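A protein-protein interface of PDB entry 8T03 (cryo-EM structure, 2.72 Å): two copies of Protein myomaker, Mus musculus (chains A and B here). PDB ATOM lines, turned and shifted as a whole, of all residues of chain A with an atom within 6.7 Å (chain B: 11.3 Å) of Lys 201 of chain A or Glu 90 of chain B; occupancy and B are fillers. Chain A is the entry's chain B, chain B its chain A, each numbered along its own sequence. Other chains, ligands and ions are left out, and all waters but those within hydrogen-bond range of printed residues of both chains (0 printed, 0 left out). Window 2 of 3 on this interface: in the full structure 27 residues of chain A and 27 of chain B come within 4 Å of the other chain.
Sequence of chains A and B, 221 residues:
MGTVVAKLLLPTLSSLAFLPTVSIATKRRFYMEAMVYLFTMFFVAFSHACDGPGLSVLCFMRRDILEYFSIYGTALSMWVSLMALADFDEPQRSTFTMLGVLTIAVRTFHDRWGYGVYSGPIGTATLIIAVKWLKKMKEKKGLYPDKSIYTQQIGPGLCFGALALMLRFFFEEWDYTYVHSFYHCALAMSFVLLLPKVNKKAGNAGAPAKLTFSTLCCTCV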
ATOM      1  N   ARG A  29     -37.195  11.816   2.201  1.00  0.00           N
ATOM      2  CA  ARG A  29     -35.745  11.920   2.528  1.00  0.00           C
ATOM      3  C   ARG A  29     -34.903  12.070   1.248  1.00  0.00           C
ATOM      4  O   ARG A  29     -33.706  11.721   1.297  1.00  0.00           O
ATOM      5  CB  ARG A  29     -35.291  10.702   3.345  1.00  0.00           C
ATOM      6  CG  ARG A  29     -36.151  10.385   4.562  1.00  0.00           C
ATOM      7  CD  ARG A  29     -35.632  11.072   5.808  1.00  0.00           C
ATOM      8  NE  ARG A  29     -34.348  10.527   6.237  1.00  0.00           N
ATOM      9  CZ  ARG A  29     -33.560  11.045   7.181  1.00  0.00           C
ATOM     10  NH1 ARG A  29     -33.908  12.148   7.827  1.00  0.00           N
ATOM     11  NH2 ARG A  29     -32.414  10.453   7.475  1.00  0.00           N
ATOM     12  N   ASP A  87     -31.650   4.684  -9.049  1.00  0.00           N
ATOM     13  CA  ASP A  87     -31.389   4.184  -7.669  1.00  0.00           C
ATOM     14  C   ASP A  87     -30.008   3.516  -7.625  1.00  0.00           C
ATOM     15  O   ASP A  87     -29.939   2.289  -7.397  1.00  0.00           O
ATOM     16  CB  ASP A  87     -32.522   3.261  -7.199  1.00  0.00           C
ATOM     17  CG  ASP A  87     -32.427   2.826  -5.743  1.00  0.00           C
ATOM     18  OD1 ASP A  87     -32.781   1.665  -5.458  1.00  0.00           O
ATOM     19  OD2 ASP A  87     -32.006   3.652  -4.906  1.00  0.00           O
ATOM     20  N   PHE A  88     -28.949   4.300  -7.846  1.00  0.00           N
ATOM     21  CA  PHE A  88     -27.538   3.829  -7.895  1.00  0.00           C
ATOM     22  C   PHE A  88     -26.960   3.734  -6.479  1.00  0.00           C
ATOM     23  O   PHE A  88     -27.398   4.491  -5.588  1.00  0.00           O
ATOM     24  CB  PHE A  88     -26.672   4.746  -8.765  1.00  0.00           C
ATOM     25  CG  PHE A  88     -26.778   4.467 -10.242  1.00  0.00           C
ATOM     26  CD1 PHE A  88     -26.143   3.365 -10.796  1.00  0.00           C
ATOM     27  CD2 PHE A  88     -27.521   5.292 -11.073  1.00  0.00           C
ATOM     28  CE1 PHE A  88     -26.242   3.098 -12.153  1.00  0.00           C
ATOM     29  CE2 PHE A  88     -27.616   5.025 -12.431  1.00  0.00           C
ATOM     30  CZ  PHE A  88     -26.978   3.928 -12.968  1.00  0.00           C
ATOM     31  N   ASP A  89     -26.009   2.841  -6.313  1.00  0.00           N
ATOM     32  CA  ASP A  89     -25.180   2.711  -5.088  1.00  0.00           C
ATOM     33  C   ASP A  89     -23.901   3.530  -5.269  1.00  0.00           C
ATOM     34  O   ASP A  89     -23.527   3.809  -6.430  1.00  0.00           O
ATOM     35  CB  ASP A  89     -24.841   1.251  -4.785  1.00  0.00           C
ATOM     36  CG  ASP A  89     -26.036   0.433  -4.330  1.00  0.00           C
ATOM     37  OD1 ASP A  89     -26.187   0.248  -3.104  1.00  0.00           O
ATOM     38  OD2 ASP A  89     -26.803  -0.018  -5.204  1.00  0.00           O
ATOM     39  N   GLU A  90     -23.255   3.876  -4.153  1.00  0.00           N
ATOM     40  CA  GLU A  90     -22.060   4.763  -4.125  1.00  0.00           C
ATOM     41  C   GLU A  90     -20.838   3.900  -4.447  1.00  0.00           C
ATOM     42  O   GLU A  90     -20.667   2.790  -3.902  1.00  0.00           O
ATOM     43  CB  GLU A  90     -21.843   5.398  -2.746  1.00  0.00           C
ATOM     44  CG  GLU A  90     -22.866   6.435  -2.343  1.00  0.00           C
ATOM     45  CD  GLU A  90     -22.722   7.793  -3.011  1.00  0.00           C
ATOM     46  OE1 GLU A  90     -23.556   8.674  -2.724  1.00  0.00           O
ATOM     47  OE2 GLU A  90     -21.785   7.970  -3.816  1.00  0.00           O
ATOM     48  N   ARG A  93     -23.512   6.789  -7.572  1.00  0.00           N
ATOM     49  CA  ARG A  93     -24.673   7.662  -7.241  1.00  0.00           C
ATOM     50  C   ARG A  93     -24.275   9.137  -7.373  1.00  0.00           C
ATOM     51  O   ARG A  93     -24.960   9.865  -8.119  1.00  0.00           O
ATOM     52  CB  ARG A  93     -25.195   7.373  -5.830  1.00  0.00           C
ATOM     53  CG  ARG A  93     -26.471   8.124  -5.481  1.00  0.00           C
ATOM     54  CD  ARG A  93     -27.133   7.556  -4.242  1.00  0.00           C
ATOM     55  NE  ARG A  93     -28.375   6.860  -4.560  1.00  0.00           N
ATOM     56  CZ  ARG A  93     -29.599   7.394  -4.531  1.00  0.00           C
ATOM     57  NH1 ARG A  93     -29.789   8.659  -4.186  1.00  0.00           N
ATOM     58  NH2 ARG A  93     -30.642   6.645  -4.848  1.00  0.00           N
ATOM     59  N   SER A  94     -23.212   9.552  -6.677  1.00  0.00           N
ATOM     60  CA  SER A  94     -22.693  10.948  -6.676  1.00  0.00           C
ATOM     61  C   SER A  94     -21.971  11.272  -7.996  1.00  0.00           C
ATOM     62  O   SER A  94     -22.045  12.444  -8.413  1.00  0.00           O
ATOM     63  CB  SER A  94     -21.806  11.213  -5.481  1.00  0.00           C
ATOM     64  OG  SER A  94     -20.922  10.126  -5.246  1.00  0.00           O
ATOM     65  N   VAL A 198     -39.407   5.984  -0.942  1.00  0.00           N
ATOM     66  CA  VAL A 198     -38.475   6.490   0.114  1.00  0.00           C
ATOM     67  C   VAL A 198     -37.034   6.392  -0.402  1.00  0.00           C
ATOM     68  O   VAL A 198     -36.738   5.448  -1.165  1.00  0.00           O
ATOM     69  CB  VAL A 198     -38.659   5.749   1.456  1.00  0.00           C
ATOM     70  CG1 VAL A 198     -38.261   4.281   1.378  1.00  0.00           C
ATOM     71  CG2 VAL A 198     -37.921   6.442   2.595  1.00  0.00           C
ATOM     72  N   ASN A 199     -36.179   7.336   0.005  1.00  0.00           N
ATOM     73  CA  ASN A 199     -34.715   7.308  -0.259  1.00  0.00           C
ATOM     74  C   ASN A 199     -34.118   6.167   0.573  1.00  0.00           C
ATOM     75  O   ASN A 199     -33.954   6.348   1.797  1.00  0.00           O
ATOM     76  CB  ASN A 199     -34.057   8.664   0.022  1.00  0.00           C
ATOM     77  CG  ASN A 199     -32.587   8.720  -0.344  1.00  0.00           C
ATOM     78  OD1 ASN A 199     -32.063   7.831  -1.014  1.00  0.00           O
ATOM     79  ND2 ASN A 199     -31.909   9.774   0.082  1.00  0.00           N
ATOM     80  N   LYS A 200     -33.821   5.036  -0.078  1.00  0.00           N
ATOM     81  CA  LYS A 200     -33.297   3.795   0.557  1.00  0.00           C
ATOM     82  C   LYS A 200     -31.872   4.012   1.090  1.00  0.00           C
ATOM     83  O   LYS A 200     -31.439   3.188   1.921  1.00  0.00           O
ATOM     84  CB  LYS A 200     -33.356   2.632  -0.439  1.00  0.00           C
ATOM     85  CG  LYS A 200     -34.758   2.096  -0.704  1.00  0.00           C
ATOM     86  CD  LYS A 200     -34.954   1.522  -2.092  1.00  0.00           C
ATOM     87  CE  LYS A 200     -34.077   0.321  -2.379  1.00  0.00           C
ATOM     88  NZ  LYS A 200     -34.131  -0.061  -3.810  1.00  0.00           N
ATOM     89  N   LYS A 201     -31.175   5.068   0.645  1.00  0.00           N
ATOM     90  CA  LYS A 201     -29.799   5.421   1.098  1.00  0.00           C
ATOM     91  C   LYS A 201     -29.844   6.387   2.295  1.00  0.00           C
ATOM     92  O   LYS A 201     -28.749   6.707   2.803  1.00  0.00           O
ATOM     93  CB  LYS A 201     -28.990   6.017  -0.062  1.00  0.00           C
ATOM     94  CG  LYS A 201     -29.055   5.265  -1.388  1.00  0.00           C
ATOM     95  CD  LYS A 201     -28.689   3.792  -1.323  1.00  0.00           C
ATOM     96  CE  LYS A 201     -28.981   3.070  -2.624  1.00  0.00           C
ATOM     97  NZ  LYS A 201     -28.724   1.614  -2.526  1.00  0.00           N
ATOM     98  N   ALA A 202     -31.031   6.842   2.729  1.00  0.00           N
ATOM     99  CA  ALA A 202     -31.218   7.748   3.894  1.00  0.00           C
ATOM    100  C   ALA A 202     -32.362   7.305   4.825  1.00  0.00           C
ATOM    101  O   ALA A 202     -32.577   8.009   5.834  1.00  0.00           O
ATOM    102  CB  ALA A 202     -31.446   9.154   3.396  1.00  0.00           C
ATOM    103  N   GLY A 203     -33.062   6.200   4.535  1.00  0.00           N
ATOM    104  CA  GLY A 203     -34.191   5.709   5.354  1.00  0.00           C
ATOM    105  C   GLY A 203     -34.743   4.386   4.847  1.00  0.00           C
ATOM    106  O   GLY A 203     -34.150   3.710   4.001  1.00  0.00           O
ATOM    107  N   PHE B  30     -12.394   8.543  -4.645  1.00  0.00           N
ATOM    108  CA  PHE B  30     -13.069   9.871  -4.650  1.00  0.00           C
ATOM    109  C   PHE B  30     -13.346  10.257  -6.108  1.00  0.00           C
ATOM    110  O   PHE B  30     -12.653  11.144  -6.652  1.00  0.00           O
ATOM    111  CB  PHE B  30     -12.228  10.936  -3.935  1.00  0.00           C
ATOM    112  CG  PHE B  30     -12.199  10.839  -2.430  1.00  0.00           C
ATOM    113  CD1 PHE B  30     -13.316  11.173  -1.678  1.00  0.00           C
ATOM    114  CD2 PHE B  30     -11.045  10.452  -1.762  1.00  0.00           C
ATOM    115  CE1 PHE B  30     -13.286  11.099  -0.291  1.00  0.00           C
ATOM    116  CE2 PHE B  30     -11.017  10.380  -0.378  1.00  0.00           C
ATOM    117  CZ  PHE B  30     -12.136  10.703   0.356  1.00  0.00           C
ATOM    118  N   MET B  32     -16.248  11.450  -7.662  1.00  0.00           N
ATOM    119  CA  MET B  32     -17.009  12.719  -7.852  1.00  0.00           C
ATOM    120  C   MET B  32     -16.055  13.918  -7.750  1.00  0.00           C
ATOM    121  O   MET B  32     -16.250  14.880  -8.516  1.00  0.00           O
ATOM    122  CB  MET B  32     -18.135  12.855  -6.819  1.00  0.00           C
ATOM    123  CG  MET B  32     -18.961  14.128  -6.963  1.00  0.00           C
ATOM    124  SD  MET B  32     -18.419  15.474  -5.875  1.00  0.00           S
ATOM    125  CE  MET B  32     -18.985  14.869  -4.286  1.00  0.00           C
ATOM    126  N   GLU B  33     -15.072  13.863  -6.844  1.00  0.00           N
ATOM    127  CA  GLU B  33     -14.024  14.909  -6.679  1.00  0.00           C
ATOM    128  C   GLU B  33     -13.093  14.876  -7.899  1.00  0.00           C
ATOM    129  O   GLU B  33     -12.756  15.964  -8.403  1.00  0.00           O
ATOM    130  CB  GLU B  33     -13.226  14.712  -5.386  1.00  0.00           C
ATOM    131  CG  GLU B  33     -13.997  15.049  -4.117  1.00  0.00           C
ATOM    132  CD  GLU B  33     -15.083  14.070  -3.696  1.00  0.00           C
ATOM    133  OE1 GLU B  33     -15.125  12.949  -4.245  1.00  0.00           O
ATOM    134  OE2 GLU B  33     -15.890  14.433  -2.817  1.00  0.00           O
ATOM    135  N   MET B  83     -15.448  19.553   1.516  1.00  0.00           N
ATOM    136  CA  MET B  83     -16.611  18.685   1.863  1.00  0.00           C
ATOM    137  C   MET B  83     -16.166  17.218   1.971  1.00  0.00           C
ATOM    138  O   MET B  83     -16.785  16.488   2.772  1.00  0.00           O
ATOM    139  CB  MET B  83     -17.750  18.814   0.845  1.00  0.00           C
ATOM    140  CG  MET B  83     -18.504  20.136   0.924  1.00  0.00           C
ATOM    141  SD  MET B  83     -19.218  20.492   2.553  1.00  0.00           S
ATOM    142  CE  MET B  83     -18.029  21.674   3.189  1.00  0.00           C
ATOM    143  N   ALA B  84     -15.149  16.799   1.206  1.00  0.00           N
ATOM    144  CA  ALA B  84     -14.491  15.474   1.334  1.00  0.00           C
ATOM    145  C   ALA B  84     -13.779  15.384   2.692  1.00  0.00           C
ATOM    146  O   ALA B  84     -13.826  14.302   3.311  1.00  0.00           O
ATOM    147  CB  ALA B  84     -13.530  15.241   0.191  1.00  0.00           C
ATOM    148  N   ALA B  86     -14.626  17.264   5.409  1.00  0.00           N
ATOM    149  CA  ALA B  86     -15.736  17.308   6.394  1.00  0.00           C
ATOM    150  C   ALA B  86     -16.289  15.893   6.621  1.00  0.00           C
ATOM    151  O   ALA B  86     -16.673  15.597   7.771  1.00  0.00           O
ATOM    152  CB  ALA B  86     -16.811  18.268   5.940  1.00  0.00           C
ATOM    153  N   ASP B  87     -16.314  15.060   5.569  1.00  0.00           N
ATOM    154  CA  ASP B  87     -16.616  13.602   5.621  1.00  0.00           C
ATOM    155  C   ASP B  87     -18.018  13.397   6.214  1.00  0.00           C
ATOM    156  O   ASP B  87     -18.127  12.808   7.309  1.00  0.00           O
ATOM    157  CB  ASP B  87     -15.520  12.848   6.386  1.00  0.00           C
ATOM    158  CG  ASP B  87     -15.651  11.332   6.360  1.00  0.00           C
ATOM    159  OD1 ASP B  87     -15.310  10.699   7.381  1.00  0.00           O
ATOM    160  OD2 ASP B  87     -16.087  10.793   5.321  1.00  0.00           O
ATOM    161  N   PHE B  88     -19.049  13.875   5.510  1.00  0.00           N
ATOM    162  CA  PHE B  88     -20.471  13.816   5.943  1.00  0.00           C
ATOM    163  C   PHE B  88     -21.076  12.450   5.596  1.00  0.00           C
ATOM    164  O   PHE B  88     -20.626  11.812   4.622  1.00  0.00           O
ATOM    165  CB  PHE B  88     -21.294  14.944   5.310  1.00  0.00           C
ATOM    166  CG  PHE B  88     -21.169  16.264   6.022  1.00  0.00           C
ATOM    167  CD1 PHE B  88     -21.828  16.480   7.224  1.00  0.00           C
ATOM    168  CD2 PHE B  88     -20.386  17.285   5.503  1.00  0.00           C
ATOM    169  CE1 PHE B  88     -21.711  17.691   7.890  1.00  0.00           C
ATOM    170  CE2 PHE B  88     -20.272  18.497   6.169  1.00  0.00           C
ATOM    171  CZ  PHE B  88     -20.934  18.696   7.361  1.00  0.00           C
ATOM    172  N   ASP B  89     -22.059  12.052   6.375  1.00  0.00           N
ATOM    173  CA  ASP B  89     -22.913  10.866   6.112  1.00  0.00           C
ATOM    174  C   ASP B  89     -24.164  11.317   5.356  1.00  0.00           C
ATOM    175  O   ASP B  89     -24.509  12.517   5.430  1.00  0.00           O
ATOM    176  CB  ASP B  89     -23.300  10.148   7.405  1.00  0.00           C
ATOM    177  CG  ASP B  89     -22.138   9.437   8.075  1.00  0.00           C
ATOM    178  OD1 ASP B  89     -22.015   8.209   7.887  1.00  0.00           O
ATOM    179  OD2 ASP B  89     -21.369  10.116   8.786  1.00  0.00           O
ATOM    180  N   GLU B  90     -24.820  10.373   4.677  1.00  0.00           N
ATOM    181  CA  GLU B  90     -25.988  10.643   3.796  1.00  0.00           C
ATOM    182  C   GLU B  90     -27.230  10.723   4.687  1.00  0.00           C
ATOM    183  O   GLU B  90     -27.443   9.875   5.579  1.00  0.00           O
ATOM    184  CB  GLU B  90     -26.213   9.525   2.770  1.00  0.00           C
ATOM    185  CG  GLU B  90     -25.166   9.425   1.684  1.00  0.00           C
ATOM    186  CD  GLU B  90     -25.258  10.472   0.587  1.00  0.00           C
ATOM    187  OE1 GLU B  90     -24.404  10.443  -0.321  1.00  0.00           O
ATOM    188  OE2 GLU B  90     -26.176  11.318   0.639  1.00  0.00           O
ATOM    189  N   PRO B  91     -28.035  11.795   4.519  1.00  0.00           N
ATOM    190  CA  PRO B  91     -28.380  12.436   3.255  1.00  0.00           C
ATOM    191  C   PRO B  91     -27.704  13.815   3.140  1.00  0.00           C
ATOM    192  O   PRO B  91     -27.913  14.463   2.133  1.00  0.00           O
ATOM    193  CB  PRO B  91     -29.903  12.539   3.322  1.00  0.00           C
ATOM    194  CG  PRO B  91     -30.177  12.786   4.792  1.00  0.00           C
ATOM    195  CD  PRO B  91     -28.987  12.224   5.567  1.00  0.00           C
ATOM    196  N   GLN B  92     -26.918  14.216   4.106  1.00  0.00           N
ATOM    197  CA  GLN B  92     -26.250  15.545   4.193  1.00  0.00           C
ATOM    198  C   GLN B  92     -25.116  15.619   3.167  1.00  0.00           C
ATOM    199  O   GLN B  92     -24.902  16.720   2.620  1.00  0.00           O
ATOM    200  CB  GLN B  92     -25.684  15.797   5.594  1.00  0.00           C
ATOM    201  CG  GLN B  92     -26.746  15.910   6.682  1.00  0.00           C
ATOM    202  CD  GLN B  92     -26.266  15.433   8.032  1.00  0.00           C
ATOM    203  OE1 GLN B  92     -26.291  16.171   9.015  1.00  0.00           O
ATOM    204  NE2 GLN B  92     -25.826  14.186   8.095  1.00  0.00           N
ATOM    205  N   ARG B  93     -24.416  14.500   2.932  1.00  0.00           N
ATOM    206  CA  ARG B  93     -23.235  14.416   2.029  1.00  0.00           C
ATOM    207  C   ARG B  93     -23.586  14.994   0.652  1.00  0.00           C
ATOM    208  O   ARG B  93     -22.871  15.911   0.201  1.00  0.00           O
ATOM    209  CB  ARG B  93     -22.748  12.971   1.890  1.00  0.00           C
ATOM    210  CG  ARG B  93     -21.457  12.831   1.097  1.00  0.00           C
ATOM    211  CD  ARG B  93     -20.835  11.462   1.282  1.00  0.00           C
ATOM    212  NE  ARG B  93     -19.609  11.524   2.070  1.00  0.00           N
ATOM    213  CZ  ARG B  93     -18.371  11.624   1.579  1.00  0.00           C
ATOM    214  NH1 ARG B  93     -18.149  11.670   0.273  1.00  0.00           N
ATOM    215  NH2 ARG B  93     -17.343  11.675   2.412  1.00  0.00           N
ATOM    216  N   SER B  94     -24.645  14.479   0.021  1.00  0.00           N
ATOM    217  CA  SER B  94     -25.125  14.913  -1.320  1.00  0.00           C
ATOM    218  C   SER B  94     -25.805  16.290  -1.244  1.00  0.00           C
ATOM    219  O   SER B  94     -25.704  17.033  -2.241  1.00  0.00           O
ATOM    220  CB  SER B  94     -26.031  13.880  -1.952  1.00  0.00           C
ATOM    221  OG  SER B  94     -26.948  13.355  -1.003  1.00  0.00           O
ATOM    222  N   THR B  95     -26.477  16.619  -0.130  1.00  0.00           N
ATOM    223  CA  THR B  95     -27.132  17.940   0.112  1.00  0.00           C
ATOM    224  C   THR B  95     -26.069  19.044   0.128  1.00  0.00           C
ATOM    225  O   THR B  95     -26.288  20.071  -0.547  1.00  0.00           O
ATOM    226  CB  THR B  95     -27.961  17.951   1.406  1.00  0.00           C
ATOM    227  OG1 THR B  95     -28.959  16.937   1.290  1.00  0.00           O
ATOM    228  CG2 THR B  95     -28.628  19.281   1.701  1.00  0.00           C
ATOM    229  N   PHE B  96     -24.978  18.849   0.877  1.00  0.00           N
ATOM    230  CA  PHE B  96     -23.863  19.827   0.991  1.00  0.00           C
ATOM    231  C   PHE B  96     -23.140  19.942  -0.356  1.00  0.00           C
ATOM    232  O   PHE B  96     -22.772  21.077  -0.696  1.00  0.00           O
ATOM    233  CB  PHE B  96     -22.905  19.483   2.137  1.00  0.00           C
ATOM    234  CG  PHE B  96     -23.388  19.917   3.499  1.00  0.00           C
ATOM    235  CD1 PHE B  96     -23.623  21.258   3.774  1.00  0.00           C
ATOM    236  CD2 PHE B  96     -23.605  18.991   4.509  1.00  0.00           C
ATOM    237  CE1 PHE B  96     -24.071  21.660   5.024  1.00  0.00           C
ATOM    238  CE2 PHE B  96     -24.049  19.395   5.760  1.00  0.00           C
ATOM    239  CZ  PHE B  96     -24.282  20.728   6.015  1.00  0.00           C
ATOM    240  N   THR B  97     -22.972  18.841  -1.101  1.00  0.00           N
ATOM    241  CA  THR B  97     -22.414  18.860  -2.484  1.00  0.00           C
ATOM    242  C   THR B  97     -23.282  19.764  -3.369  1.00  0.00           C
ATOM    243  O   THR B  97     -22.713  20.658  -4.024  1.00  0.00           O
ATOM    244  CB  THR B  97     -22.283  17.457  -3.095  1.00  0.00           C
ATOM    245  OG1 THR B  97     -21.487  16.661  -2.218  1.00  0.00           O
ATOM    246  CG2 THR B  97     -21.658  17.477  -4.476  1.00  0.00           C
ATOM    247  N   MET B  98     -24.600  19.543  -3.366  1.00  0.00           N
ATOM    248  CA  MET B  98     -25.586  20.263  -4.221  1.00  0.00           C
ATOM    249  C   MET B  98     -25.651  21.746  -3.824  1.00  0.00           C
ATOM    250  O   MET B  98     -25.848  22.579  -4.728  1.00  0.00           O
ATOM    251  CB  MET B  98     -26.980  19.636  -4.093  1.00  0.00           C
ATOM    252  CG  MET B  98     -27.921  19.969  -5.241  1.00  0.00           C
ATOM    253  SD  MET B  98     -27.487  19.142  -6.795  1.00  0.00           S
ATOM    254  CE  MET B  98     -26.992  20.552  -7.785  1.00  0.00           C
ATOM    255  N   LEU B  99     -25.494  22.055  -2.531  1.00  0.00           N
ATOM    256  CA  LEU B  99     -25.501  23.440  -1.978  1.00  0.00           C
ATOM    257  C   LEU B  99     -24.362  24.254  -2.604  1.00  0.00           C
ATOM    258  O   LEU B  99     -24.643  25.369  -3.083  1.00  0.00           O
ATOM    259  CB  LEU B  99     -25.372  23.362  -0.453  1.00  0.00           C
ATOM    260  CG  LEU B  99     -25.329  24.692   0.296  1.00  0.00           C
ATOM    261  CD1 LEU B  99     -26.661  25.422   0.233  1.00  0.00           C
ATOM    262  CD2 LEU B  99     -24.913  24.463   1.742  1.00  0.00           C
ATOM    263  N   LYS B 132     -18.810  21.124  12.843  1.00  0.00           N
ATOM    264  CA  LYS B 132     -18.846  19.638  12.932  1.00  0.00           C
ATOM    265  C   LYS B 132     -17.759  19.152  13.902  1.00  0.00           C
ATOM    266  O   LYS B 132     -18.087  18.316  14.767  1.00  0.00           O
ATOM    267  CB  LYS B 132     -18.678  18.939  11.577  1.00  0.00           C
ATOM    268  CG  LYS B 132     -18.654  17.421  11.704  1.00  0.00           C
ATOM    269  CD  LYS B 132     -18.613  16.619  10.432  1.00  0.00           C
ATOM    270  CE  LYS B 132     -18.380  15.157  10.757  1.00  0.00           C
ATOM    271  NZ  LYS B 132     -18.442  14.290   9.560  1.00  0.00           N
ATOM    272  N   ASN B 199     -11.856   7.083   0.408  1.00  0.00           N
ATOM    273  CA  ASN B 199     -13.314   7.367   0.484  1.00  0.00           C
ATOM    274  C   ASN B 199     -13.961   6.247   1.307  1.00  0.00           C
ATOM    275  O   ASN B 199     -14.144   5.140   0.760  1.00  0.00           O
ATOM    276  CB  ASN B 199     -13.937   7.527  -0.907  1.00  0.00           C
ATOM    277  CG  ASN B 199     -15.398   7.937  -0.882  1.00  0.00           C
ATOM    278  OD1 ASN B 199     -15.933   8.320   0.157  1.00  0.00           O
ATOM    279  ND2 ASN B 199     -16.052   7.869  -2.030  1.00  0.00           N
ATOM    280  N   LYS B 200     -14.277   6.534   2.575  1.00  0.00           N
ATOM    281  CA  LYS B 200     -14.851   5.570   3.554  1.00  0.00           C
ATOM    282  C   LYS B 200     -16.279   5.168   3.154  1.00  0.00           C
ATOM    283  O   LYS B 200     -16.753   4.140   3.680  1.00  0.00           O
ATOM    284  CB  LYS B 200     -14.805   6.167   4.965  1.00  0.00           C
ATOM    285  CG  LYS B 200     -13.414   6.217   5.586  1.00  0.00           C
ATOM    286  CD  LYS B 200     -13.206   7.361   6.557  1.00  0.00           C
ATOM    287  CE  LYS B 200     -14.113   7.299   7.768  1.00  0.00           C
ATOM    288  NZ  LYS B 200     -14.042   8.547   8.563  1.00  0.00           N
ATOM    289  N   LYS B 201     -16.936   5.931   2.269  1.00  0.00           N
ATOM    290  CA  LYS B 201     -18.309   5.646   1.765  1.00  0.00           C
ATOM    291  C   LYS B 201     -18.262   4.796   0.482  1.00  0.00           C
ATOM    292  O   LYS B 201     -19.357   4.440   0.000  1.00  0.00           O
ATOM    293  CB  LYS B 201     -19.077   6.954   1.530  1.00  0.00           C
ATOM    294  CG  LYS B 201     -19.006   7.989   2.651  1.00  0.00           C
ATOM    295  CD  LYS B 201     -19.416   7.494   4.027  1.00  0.00           C
ATOM    296  CE  LYS B 201     -19.120   8.507   5.113  1.00  0.00           C
ATOM    297  NZ  LYS B 201     -19.422   7.983   6.466  1.00  0.00           N
ATOM    298  N   ALA B 202     -17.071   4.488  -0.058  1.00  0.00           N
ATOM    299  CA  ALA B 202     -16.883   3.644  -1.269  1.00  0.00           C
ATOM    300  C   ALA B 202     -15.772   2.591  -1.103  1.00  0.00           C
ATOM    301  O   ALA B 202     -15.557   1.835  -2.074  1.00  0.00           O
ATOM    302  CB  ALA B 202     -16.604   4.536  -2.455  1.00  0.00           C
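The side-chain carboxylate of Glu 90 of chain B sits close to the side-chain carboxylate of Glu 90 of chain A.
The side-chain hydroxyl of Ser 94 of chain A is in hydrogen-bond range of the side-chain carboxylate of Glu 90 of chain A, 2.7 Å away. OD1 of Asn 199 of chain B sits close to N of Lys 201 of chain B. The side-chain carboxylate (OE2) of Glu 90 of chain B is in hydrogen-bond range of the side-chain hydroxyl (OG) of Ser 94 of chain B, at 2.7 Å. O of Pro 91 of chain B lies within hydrogen-bond range of OG1 of Thr 95 of chain B (2.8 Å). The side-chain carboxylate (OD1) of Asp 89 of chain A is in salt-bridge range of the side-chain amino group (NZ) of Lys 201 of chain A (2.9 Å). OD1 of Asp 89 of chain B is in salt-bridge range of NZ of Lys 201 of chain B (3.0 Å).
Among the printed residues, merely in contact across the chains: Glu 90 of chain A with Lys 201 of chain B (3.8 Å), Ser 94 of chain A with Met 32 of chain B (3.8 Å), Lys 201 of chain A with Glu 90 of chain B (3.8 Å) and Ala 202 of chain A with Pro 91 of chain B (3.7 Å).
Of the printed residues of chain B, Ser 94 of chain A touches Met 32. No residue of chain B comes within 4 Å of Asn 199 of chain A. Lys 201 of chain A touches one residue of chain B. No residue of chain B comes within 4 Å of Gly 203 of chain A. Printed residues of chain A within 4 Å of Met 32 of chain B: Ser 94. Of the printed residues of chain A, Pro 91 of chain B touches Ala 202 (3.7 Å). Thr 95 of chain B touches none of the printed residues of chain A. Printed residues of chain A within 4 Å of Lys 201 of chain B: Glu 90. The nearest residue of chain A that does not touch Glu 90 of chain B is Ala 202 of chain A (4.6 Å).
Of the 24 printed residues of chain B, 4 touch a printed residue of chain A. Of the 13 printed residues of chain A, 4 touch a printed residue of chain B. Hydrophobic or aromatic side chains of chain A that line the printed part of chain B: Ala 202. Among the printed residues, 5 pairs touch across the chains. Among the printed residues, no Asp or Glu carboxylate lies within 4 Å of a Lys or Arg side-chain nitrogen of the other chain.
Glu 90 of chain B touches its own counterpart, Glu 90 of chain A. Glu 90 of chain A touches Lys 201 of chain B, and with the chains exchanged Lys 201 of chain A touches Glu 90 of chain B. Positions printed for both chains: 87, 88, 89, 90, 93, 94, 199, 200, 201 and 202. Of the 5 pairs that touch across the chains among the printed residues, 3 have their exchanged pair printed and touching as well.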
